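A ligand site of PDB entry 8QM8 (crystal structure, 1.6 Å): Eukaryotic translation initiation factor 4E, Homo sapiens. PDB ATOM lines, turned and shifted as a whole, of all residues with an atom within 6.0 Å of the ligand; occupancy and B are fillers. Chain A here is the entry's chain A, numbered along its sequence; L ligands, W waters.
The indole nitrogen (NE1) of Trp 128 lies close to a fluorine (F1) of the ligand. Merely in contact with the ligand: Ser 81, Tyr 89, Leu 43, Ile 77, Leu 132, Phe 70, Leu 83, Leu 73, Asn 82, Gln 78, Val 152 and Leu 124. Hydrophobic or aromatic side chains within 4 Å of the ligand: Leu 43, Phe 70, Leu 73, Tyr 74, Ile 77, Leu 83, Tyr 89, Leu 124, Trp 128, Leu 132 and Val 152.
The side-chain hydroxyl (OG) of Ser 81 lies within hydrogen-bond range of the backbone carbonyl oxygen (O) of Ile 77, at 2.5 Å. The side-chain hydroxyl (OH) of Tyr 89 is in hydrogen-bond range of the backbone carbonyl oxygen (O) of Asn 82 (2.8 Å). N of Val 152 sits at hydrogen-bond distance from O of Tyr 89, 2.9 Å away.
Water W2 lies within hydrogen-bond range of the backbone carbonyl oxygen (O) of Asp 125 (2.7 Å), the side-chain hydroxyl (OH) of Tyr 74 (2.7 Å) and an oxygen (O2) of the ligand (2.9 Å). Water W1 lies within hydrogen-bond range of OD1 of Asp 125 and O1 of the ligand.
O2 of the ligand lies within hydrogen-bond range of OD1 of Asp 125 (2.8 Å). OH of Tyr 74 sits at hydrogen-bond distance from O3 of the ligand, 3.5 Å away.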
ATOM      1  N   LEU A  43      -1.413 -28.218 -19.134  1.00  0.00           N
ATOM      2  CA  LEU A  43      -2.209 -27.150 -19.703  1.00  0.00           C
ATOM      3  C   LEU A  43      -1.480 -25.800 -19.676  1.00  0.00           C
ATOM      4  O   LEU A  43      -0.999 -25.350 -18.613  1.00  0.00           O
ATOM      5  CB  LEU A  43      -3.508 -27.013 -18.908  1.00  0.00           C
ATOM      6  CG  LEU A  43      -4.466 -25.880 -19.400  1.00  0.00           C
ATOM      7  CD1 LEU A  43      -4.989 -26.145 -20.830  1.00  0.00           C
ATOM      8  CD2 LEU A  43      -5.640 -25.741 -18.453  1.00  0.00           C
ATOM      9  N   PHE A  64      -1.623 -32.627 -14.819  1.00  0.00           N
ATOM     10  CA  PHE A  64      -2.439 -33.650 -14.217  1.00  0.00           C
ATOM     11  C   PHE A  64      -2.188 -34.975 -14.857  1.00  0.00           C
ATOM     12  O   PHE A  64      -1.693 -35.028 -15.969  1.00  0.00           O
ATOM     13  CB  PHE A  64      -3.956 -33.331 -14.258  1.00  0.00           C
ATOM     14  CG  PHE A  64      -4.445 -33.166 -15.666  1.00  0.00           C
ATOM     15  CD1 PHE A  64      -4.908 -34.259 -16.399  1.00  0.00           C
ATOM     16  CD2 PHE A  64      -4.429 -31.946 -16.282  1.00  0.00           C
ATOM     17  CE1 PHE A  64      -5.312 -34.116 -17.708  1.00  0.00           C
ATOM     18  CE2 PHE A  64      -4.817 -31.808 -17.607  1.00  0.00           C
ATOM     19  CZ  PHE A  64      -5.267 -32.907 -18.304  1.00  0.00           C
ATOM     20  N   PHE A  70      -8.116 -34.226 -13.948  1.00  0.00           N
ATOM     21  CA  PHE A  70      -8.540 -33.558 -15.183  1.00  0.00           C
ATOM     22  C   PHE A  70      -9.879 -32.824 -14.908  1.00  0.00           C
ATOM     23  O   PHE A  70      -9.996 -31.620 -15.201  1.00  0.00           O
ATOM     24  CB  PHE A  70      -8.725 -34.590 -16.293  1.00  0.00           C
ATOM     25  CG  PHE A  70      -9.553 -34.035 -17.422  1.00  0.00           C
ATOM     26  CD1 PHE A  70      -8.995 -33.168 -18.356  1.00  0.00           C
ATOM     27  CD2 PHE A  70     -10.889 -34.342 -17.536  1.00  0.00           C
ATOM     28  CE1 PHE A  70      -9.776 -32.652 -19.381  1.00  0.00           C
ATOM     29  CE2 PHE A  70     -11.667 -33.814 -18.555  1.00  0.00           C
ATOM     30  CZ  PHE A  70     -11.100 -32.944 -19.468  1.00  0.00           C
ATOM     31  N   LEU A  73      -9.564 -29.723 -12.643  1.00  0.00           N
ATOM     32  CA  LEU A  73      -9.024 -28.619 -13.435  1.00  0.00           C
ATOM     33  C   LEU A  73     -10.084 -28.051 -14.375  1.00  0.00           C
ATOM     34  O   LEU A  73     -10.303 -26.860 -14.410  1.00  0.00           O
ATOM     35  CB  LEU A  73      -7.796 -29.074 -14.193  1.00  0.00           C
ATOM     36  CG  LEU A  73      -7.111 -27.979 -15.019  1.00  0.00           C
ATOM     37  CD1 LEU A  73      -6.592 -26.772 -14.086  1.00  0.00           C
ATOM     38  CD2 LEU A  73      -5.955 -28.514 -15.819  1.00  0.00           C
ATOM     39  N   TYR A  74     -10.811 -28.904 -15.066  1.00  0.00           N
ATOM     40  CA  TYR A  74     -11.875 -28.520 -15.989  1.00  0.00           C
ATOM     41  C   TYR A  74     -12.906 -27.678 -15.280  1.00  0.00           C
ATOM     42  O   TYR A  74     -13.230 -26.582 -15.718  1.00  0.00           O
ATOM     43  CB  TYR A  74     -12.513 -29.747 -16.614  1.00  0.00           C
ATOM     44  CG  TYR A  74     -13.461 -29.410 -17.737  1.00  0.00           C
ATOM     45  CD1 TYR A  74     -13.007 -29.282 -19.032  1.00  0.00           C
ATOM     46  CD2 TYR A  74     -14.800 -29.137 -17.494  1.00  0.00           C
ATOM     47  CE1 TYR A  74     -13.866 -28.924 -20.078  1.00  0.00           C
ATOM     48  CE2 TYR A  74     -15.675 -28.817 -18.539  1.00  0.00           C
ATOM     49  CZ  TYR A  74     -15.196 -28.690 -19.815  1.00  0.00           C
ATOM     50  OH  TYR A  74     -16.026 -28.321 -20.835  1.00  0.00           O
ATOM     51  N   ILE A  77     -11.385 -24.267 -14.302  1.00  0.00           N
ATOM     52  CA  ILE A  77     -11.249 -23.406 -15.492  1.00  0.00           C
ATOM     53  C   ILE A  77     -12.614 -22.902 -15.930  1.00  0.00           C
ATOM     54  O   ILE A  77     -12.768 -21.742 -16.319  1.00  0.00           O
ATOM     55  CB  ILE A  77     -10.554 -24.152 -16.671  1.00  0.00           C
ATOM     56  CG1 ILE A  77      -9.111 -24.527 -16.340  1.00  0.00           C
ATOM     57  CG2 ILE A  77     -10.640 -23.331 -17.970  1.00  0.00           C
ATOM     58  CD1 ILE A  77      -8.211 -23.420 -15.942  1.00  0.00           C
ATOM     59  N   GLN A  78     -13.605 -23.766 -15.862  1.00  0.00           N
ATOM     60  CA  GLN A  78     -14.974 -23.415 -16.234  1.00  0.00           C
ATOM     61  C   GLN A  78     -15.482 -22.237 -15.359  1.00  0.00           C
ATOM     62  O   GLN A  78     -16.314 -21.485 -15.822  1.00  0.00           O
ATOM     63  CB  GLN A  78     -15.892 -24.647 -16.161  1.00  0.00           C
ATOM     64  CG  GLN A  78     -17.259 -24.534 -16.873  1.00  0.00           C
ATOM     65  CD  GLN A  78     -18.061 -25.819 -16.752  1.00  0.00           C
ATOM     66  OE1 GLN A  78     -17.836 -26.663 -15.890  1.00  0.00           O
ATOM     67  NE2 GLN A  78     -19.021 -26.028 -17.628  1.00  0.00           N
ATOM     68  N   SER A  80     -13.001 -20.073 -13.505  1.00  0.00           N
ATOM     69  CA  SER A  80     -11.931 -19.074 -13.468  1.00  0.00           C
ATOM     70  C   SER A  80     -10.984 -19.231 -14.651  1.00  0.00           C
ATOM     71  O   SER A  80     -10.074 -20.071 -14.641  1.00  0.00           O
ATOM     72  CB  SER A  80     -11.145 -19.166 -12.170  1.00  0.00           C
ATOM     73  OG  SER A  80     -10.349 -20.342 -12.068  1.00  0.00           O
ATOM     74  N   SER A  81     -11.202 -18.402 -15.684  1.00  0.00           N
ATOM     75  CA  SER A  81     -10.302 -18.331 -16.831  1.00  0.00           C
ATOM     76  C   SER A  81     -10.844 -17.401 -17.901  1.00  0.00           C
ATOM     77  O   SER A  81     -12.062 -17.244 -18.008  1.00  0.00           O
ATOM     78  CB  SER A  81     -10.145 -19.704 -17.441  1.00  0.00           C
ATOM     79  OG  SER A  81     -11.442 -20.183 -17.777  1.00  0.00           O
ATOM     80  N   ASN A  82      -9.954 -16.816 -18.718  1.00  0.00           N
ATOM     81  CA  ASN A  82     -10.327 -15.791 -19.690  1.00  0.00           C
ATOM     82  C   ASN A  82     -10.738 -16.509 -20.969  1.00  0.00           C
ATOM     83  O   ASN A  82      -9.998 -17.360 -21.477  1.00  0.00           O
ATOM     84  CB  ASN A  82      -9.130 -14.845 -19.925  1.00  0.00           C
ATOM     85  CG  ASN A  82      -9.445 -13.454 -20.444  1.00  0.00           C
ATOM     86  OD1 ASN A  82      -8.818 -12.967 -21.395  1.00  0.00           O
ATOM     87  ND2 ASN A  82     -10.387 -12.747 -19.827  1.00  0.00           N
ATOM     88  N   LEU A  83     -11.920 -16.180 -21.478  1.00  0.00           N
ATOM     89  CA  LEU A  83     -12.362 -16.609 -22.792  1.00  0.00           C
ATOM     90  C   LEU A  83     -12.533 -15.329 -23.549  1.00  0.00           C
ATOM     91  O   LEU A  83     -13.645 -14.811 -23.640  1.00  0.00           O
ATOM     92  CB  LEU A  83     -13.699 -17.391 -22.746  1.00  0.00           C
ATOM     93  CG  LEU A  83     -14.228 -17.884 -24.124  1.00  0.00           C
ATOM     94  CD1 LEU A  83     -13.479 -19.043 -24.593  1.00  0.00           C
ATOM     95  CD2 LEU A  83     -15.696 -18.245 -24.070  1.00  0.00           C
ATOM     96  N   TYR A  89      -5.306 -21.810 -25.584  1.00  0.00           N
ATOM     97  CA  TYR A  89      -5.073 -22.794 -24.551  1.00  0.00           C
ATOM     98  C   TYR A  89      -4.555 -24.048 -25.207  1.00  0.00           C
ATOM     99  O   TYR A  89      -4.994 -24.374 -26.289  1.00  0.00           O
ATOM    100  CB  TYR A  89      -6.346 -23.128 -23.783  1.00  0.00           C
ATOM    101  CG  TYR A  89      -6.811 -22.010 -22.854  1.00  0.00           C
ATOM    102  CD1 TYR A  89      -7.629 -21.017 -23.320  1.00  0.00           C
ATOM    103  CD2 TYR A  89      -6.449 -21.997 -21.514  1.00  0.00           C
ATOM    104  CE1 TYR A  89      -8.129 -20.039 -22.451  1.00  0.00           C
ATOM    105  CE2 TYR A  89      -6.929 -21.033 -20.646  1.00  0.00           C
ATOM    106  CZ  TYR A  89      -7.761 -20.045 -21.126  1.00  0.00           C
ATOM    107  OH  TYR A  89      -8.187 -19.061 -20.248  1.00  0.00           O
ATOM    108  N   SER A  90      -3.610 -24.707 -24.598  1.00  0.00           N
ATOM    109  CA  SER A  90      -2.964 -25.870 -25.215  1.00  0.00           C
ATOM    110  C   SER A  90      -2.836 -26.958 -24.180  1.00  0.00           C
ATOM    111  O   SER A  90      -2.349 -26.689 -23.066  1.00  0.00           O
ATOM    112  CB  SER A  90      -1.579 -25.510 -25.702  1.00  0.00           C
ATOM    113  OG  SER A  90      -1.587 -24.431 -26.619  1.00  0.00           O
ATOM    114  N   LEU A  91      -3.222 -28.202 -24.519  1.00  0.00           N
ATOM    115  CA  LEU A  91      -2.987 -29.321 -23.620  1.00  0.00           C
ATOM    116  C   LEU A  91      -1.993 -30.220 -24.311  1.00  0.00           C
ATOM    117  O   LEU A  91      -2.322 -30.751 -25.386  1.00  0.00           O
ATOM    118  CB  LEU A  91      -4.252 -30.134 -23.331  1.00  0.00           C
ATOM    119  CG  LEU A  91      -4.040 -31.212 -22.253  1.00  0.00           C
ATOM    120  CD1 LEU A  91      -3.877 -30.602 -20.888  1.00  0.00           C
ATOM    121  CD2 LEU A  91      -5.168 -32.255 -22.271  1.00  0.00           C
ATOM    122  N   LEU A 124     -18.259 -24.505 -29.498  1.00  0.00           N
ATOM    123  CA  LEU A 124     -16.847 -24.412 -29.105  1.00  0.00           C
ATOM    124  C   LEU A 124     -16.561 -25.272 -27.872  1.00  0.00           C
ATOM    125  O   LEU A 124     -15.601 -26.050 -27.880  1.00  0.00           O
ATOM    126  CB  LEU A 124     -16.339 -22.979 -28.883  1.00  0.00           C
ATOM    127  CG  LEU A 124     -14.853 -22.836 -28.468  1.00  0.00           C
ATOM    128  CD1 LEU A 124     -13.877 -23.164 -29.646  1.00  0.00           C
ATOM    129  CD2 LEU A 124     -14.572 -21.368 -27.994  1.00  0.00           C
ATOM    130  N   ASP A 125     -17.369 -25.155 -26.841  1.00  0.00           N
ATOM    131  CA  ASP A 125     -17.157 -25.884 -25.610  1.00  0.00           C
ATOM    132  C   ASP A 125     -17.282 -27.393 -25.870  1.00  0.00           C
ATOM    133  O   ASP A 125     -16.437 -28.131 -25.365  1.00  0.00           O
ATOM    134  CB  ASP A 125     -18.168 -25.449 -24.544  1.00  0.00           C
ATOM    135  CG  ASP A 125     -18.011 -24.040 -24.017  1.00  0.00           C
ATOM    136  OD1 ASP A 125     -16.886 -23.489 -24.108  1.00  0.00           O
ATOM    137  OD2 ASP A 125     -18.986 -23.505 -23.494  1.00  0.00           O
ATOM    138  N   ARG A 126     -18.276 -27.853 -26.670  1.00  0.00           N
ATOM    139  CA  ARG A 126     -18.475 -29.277 -26.790  1.00  0.00           C
ATOM    140  C   ARG A 126     -17.354 -29.834 -27.665  1.00  0.00           C
ATOM    141  O   ARG A 126     -16.844 -30.888 -27.342  1.00  0.00           O
ATOM    142  CB  ARG A 126     -19.876 -29.696 -27.280  1.00  0.00           C
ATOM    143  CG  ARG A 126     -20.146 -29.489 -28.700  1.00  0.00           C
ATOM    144  CD  ARG A 126     -21.669 -29.660 -28.956  1.00  0.00           C
ATOM    145  NE  ARG A 126     -22.018 -29.505 -30.376  1.00  0.00           N
ATOM    146  CZ  ARG A 126     -21.770 -30.417 -31.318  1.00  0.00           C
ATOM    147  NH1 ARG A 126     -21.172 -31.566 -31.009  1.00  0.00           N
ATOM    148  NH2 ARG A 126     -22.125 -30.193 -32.575  1.00  0.00           N
ATOM    149  N   TRP A 128     -14.247 -28.624 -28.004  1.00  0.00           N
ATOM    150  CA  TRP A 128     -13.003 -28.626 -27.170  1.00  0.00           C
ATOM    151  C   TRP A 128     -13.020 -29.759 -26.172  1.00  0.00           C
ATOM    152  O   TRP A 128     -12.030 -30.506 -26.055  1.00  0.00           O
ATOM    153  CB  TRP A 128     -12.787 -27.251 -26.540  1.00  0.00           C
ATOM    154  CG  TRP A 128     -11.546 -27.114 -25.729  1.00  0.00           C
ATOM    155  CD1 TRP A 128     -11.467 -26.770 -24.426  1.00  0.00           C
ATOM    156  CD2 TRP A 128     -10.181 -27.266 -26.188  1.00  0.00           C
ATOM    157  NE1 TRP A 128     -10.172 -26.668 -24.030  1.00  0.00           N
ATOM    158  CE2 TRP A 128      -9.348 -26.993 -25.089  1.00  0.00           C
ATOM    159  CE3 TRP A 128      -9.599 -27.690 -27.417  1.00  0.00           C
ATOM    160  CZ2 TRP A 128      -7.966 -27.104 -25.166  1.00  0.00           C
ATOM    161  CZ3 TRP A 128      -8.228 -27.752 -27.487  1.00  0.00           C
ATOM    162  CH2 TRP A 128      -7.421 -27.467 -26.379  1.00  0.00           C
ATOM    163  N   LEU A 129     -14.135 -29.945 -25.468  1.00  0.00           N
ATOM    164  CA  LEU A 129     -14.229 -31.063 -24.513  1.00  0.00           C
ATOM    165  C   LEU A 129     -14.000 -32.406 -25.215  1.00  0.00           C
ATOM    166  O   LEU A 129     -13.201 -33.192 -24.749  1.00  0.00           O
ATOM    167  CB  LEU A 129     -15.533 -31.066 -23.767  1.00  0.00           C
ATOM    168  CG  LEU A 129     -15.706 -32.205 -22.763  1.00  0.00           C
ATOM    169  CD1 LEU A 129     -14.536 -32.314 -21.759  1.00  0.00           C
ATOM    170  CD2 LEU A 129     -17.082 -32.030 -22.069  1.00  0.00           C
ATOM    171  N   LEU A 132     -10.380 -32.857 -25.808  1.00  0.00           N
ATOM    172  CA  LEU A 132      -9.641 -33.191 -24.546  1.00  0.00           C
ATOM    173  C   LEU A 132      -9.852 -34.673 -24.182  1.00  0.00           C
ATOM    174  O   LEU A 132      -8.893 -35.354 -23.779  1.00  0.00           O
ATOM    175  CB  LEU A 132     -10.121 -32.308 -23.429  1.00  0.00           C
ATOM    176  CG  LEU A 132      -9.888 -30.800 -23.597  1.00  0.00           C
ATOM    177  CD1 LEU A 132     -10.569 -30.059 -22.448  1.00  0.00           C
ATOM    178  CD2 LEU A 132      -8.409 -30.501 -23.623  1.00  0.00           C
ATOM    179  N   VAL A 152      -6.518 -24.648 -28.693  1.00  0.00           N
ATOM    180  CA  VAL A 152      -7.730 -23.894 -29.061  1.00  0.00           C
ATOM    181  C   VAL A 152      -7.278 -22.411 -29.183  1.00  0.00           C
ATOM    182  O   VAL A 152      -6.608 -21.874 -28.271  1.00  0.00           O
ATOM    183  CB  VAL A 152      -8.969 -24.101 -28.134  1.00  0.00           C
ATOM    184  CG1 VAL A 152      -8.640 -23.815 -26.652  1.00  0.00           C
ATOM    185  CG2 VAL A 152     -10.137 -23.273 -28.641  1.00  0.00           C
ATOM    186  N   VAL A 154      -8.926 -18.758 -29.677  1.00  0.00           N
ATOM    187  CA  VAL A 154     -10.155 -17.956 -29.583  1.00  0.00           C
ATOM    188  C   VAL A 154      -9.924 -16.661 -30.373  1.00  0.00           C
ATOM    189  O   VAL A 154      -9.042 -15.891 -30.020  1.00  0.00           O
ATOM    190  CB  VAL A 154     -10.488 -17.634 -28.125  1.00  0.00           C
ATOM    191  CG1 VAL A 154     -11.746 -16.780 -28.050  1.00  0.00           C
ATOM    192  CG2 VAL A 154     -10.689 -18.929 -27.337  1.00  0.00           C
HETATM  193  C1  LIG L   1     -10.710 -20.958 -20.342  1.00  0.00           C
HETATM  194  C2  LIG L   1     -11.850 -21.541 -21.008  1.00  0.00           C
HETATM  195  C3  LIG L   1     -11.449 -22.432 -22.190  1.00  0.00           C
HETATM  196  C4  LIG L   1     -12.453 -23.231 -24.264  1.00  0.00           C
HETATM  197  C5  LIG L   1     -11.870 -22.215 -25.222  1.00  0.00           C
HETATM  198  C6  LIG L   1     -13.801 -23.802 -24.736  1.00  0.00           C
HETATM  199  C7  LIG L   1      -9.499 -23.955 -21.727  1.00  0.00           C
HETATM  200  C8  LIG L   1      -8.931 -25.120 -21.224  1.00  0.00           C
HETATM  201  C9  LIG L   1      -9.711 -26.097 -20.618  1.00  0.00           C
HETATM  202  C10 LIG L   1     -11.085 -25.865 -20.535  1.00  0.00           C
HETATM  203  C11 LIG L   1     -11.673 -24.698 -20.987  1.00  0.00           C
HETATM  204  C12 LIG L   1     -13.953 -25.345 -20.168  1.00  0.00           C
HETATM  205  C13 LIG L   1      -9.109 -27.335 -20.060  1.00  0.00           C
HETATM  206  C14 LIG L   1      -8.907 -28.885 -18.211  1.00  0.00           C
HETATM  207  C15 LIG L   1      -7.944 -29.604 -18.894  1.00  0.00           C
HETATM  208  C16 LIG L   1      -7.556 -29.191 -20.136  1.00  0.00           C
HETATM  209  C17 LIG L   1      -8.125 -28.079 -20.695  1.00  0.00           C
HETATM  210  O1  LIG L   1     -12.663 -22.601 -23.003  1.00  0.00           O
HETATM  211  O2  LIG L   1     -14.365 -24.662 -23.738  1.00  0.00           O
HETATM  212  C18 LIG L   1     -10.882 -23.748 -21.671  1.00  0.00           C
HETATM  213  N1  LIG L   1     -13.028 -24.492 -20.884  1.00  0.00           N
HETATM  214  C19 LIG L   1     -15.382 -24.810 -20.239  1.00  0.00           C
HETATM  215  O3  LIG L   1     -15.903 -24.937 -21.557  1.00  0.00           O
HETATM  216  C20 LIG L   1      -9.480 -27.764 -18.784  1.00  0.00           C
HETATM  217  F1  LIG L   1      -7.718 -27.671 -21.911  1.00  0.00           F
HETATM  218  O   HOH W   1     -15.441 -21.821 -22.192  1.00  0.00           O
HETATM  219  O   HOH W   2     -14.991 -27.389 -23.185  1.00  0.00           O
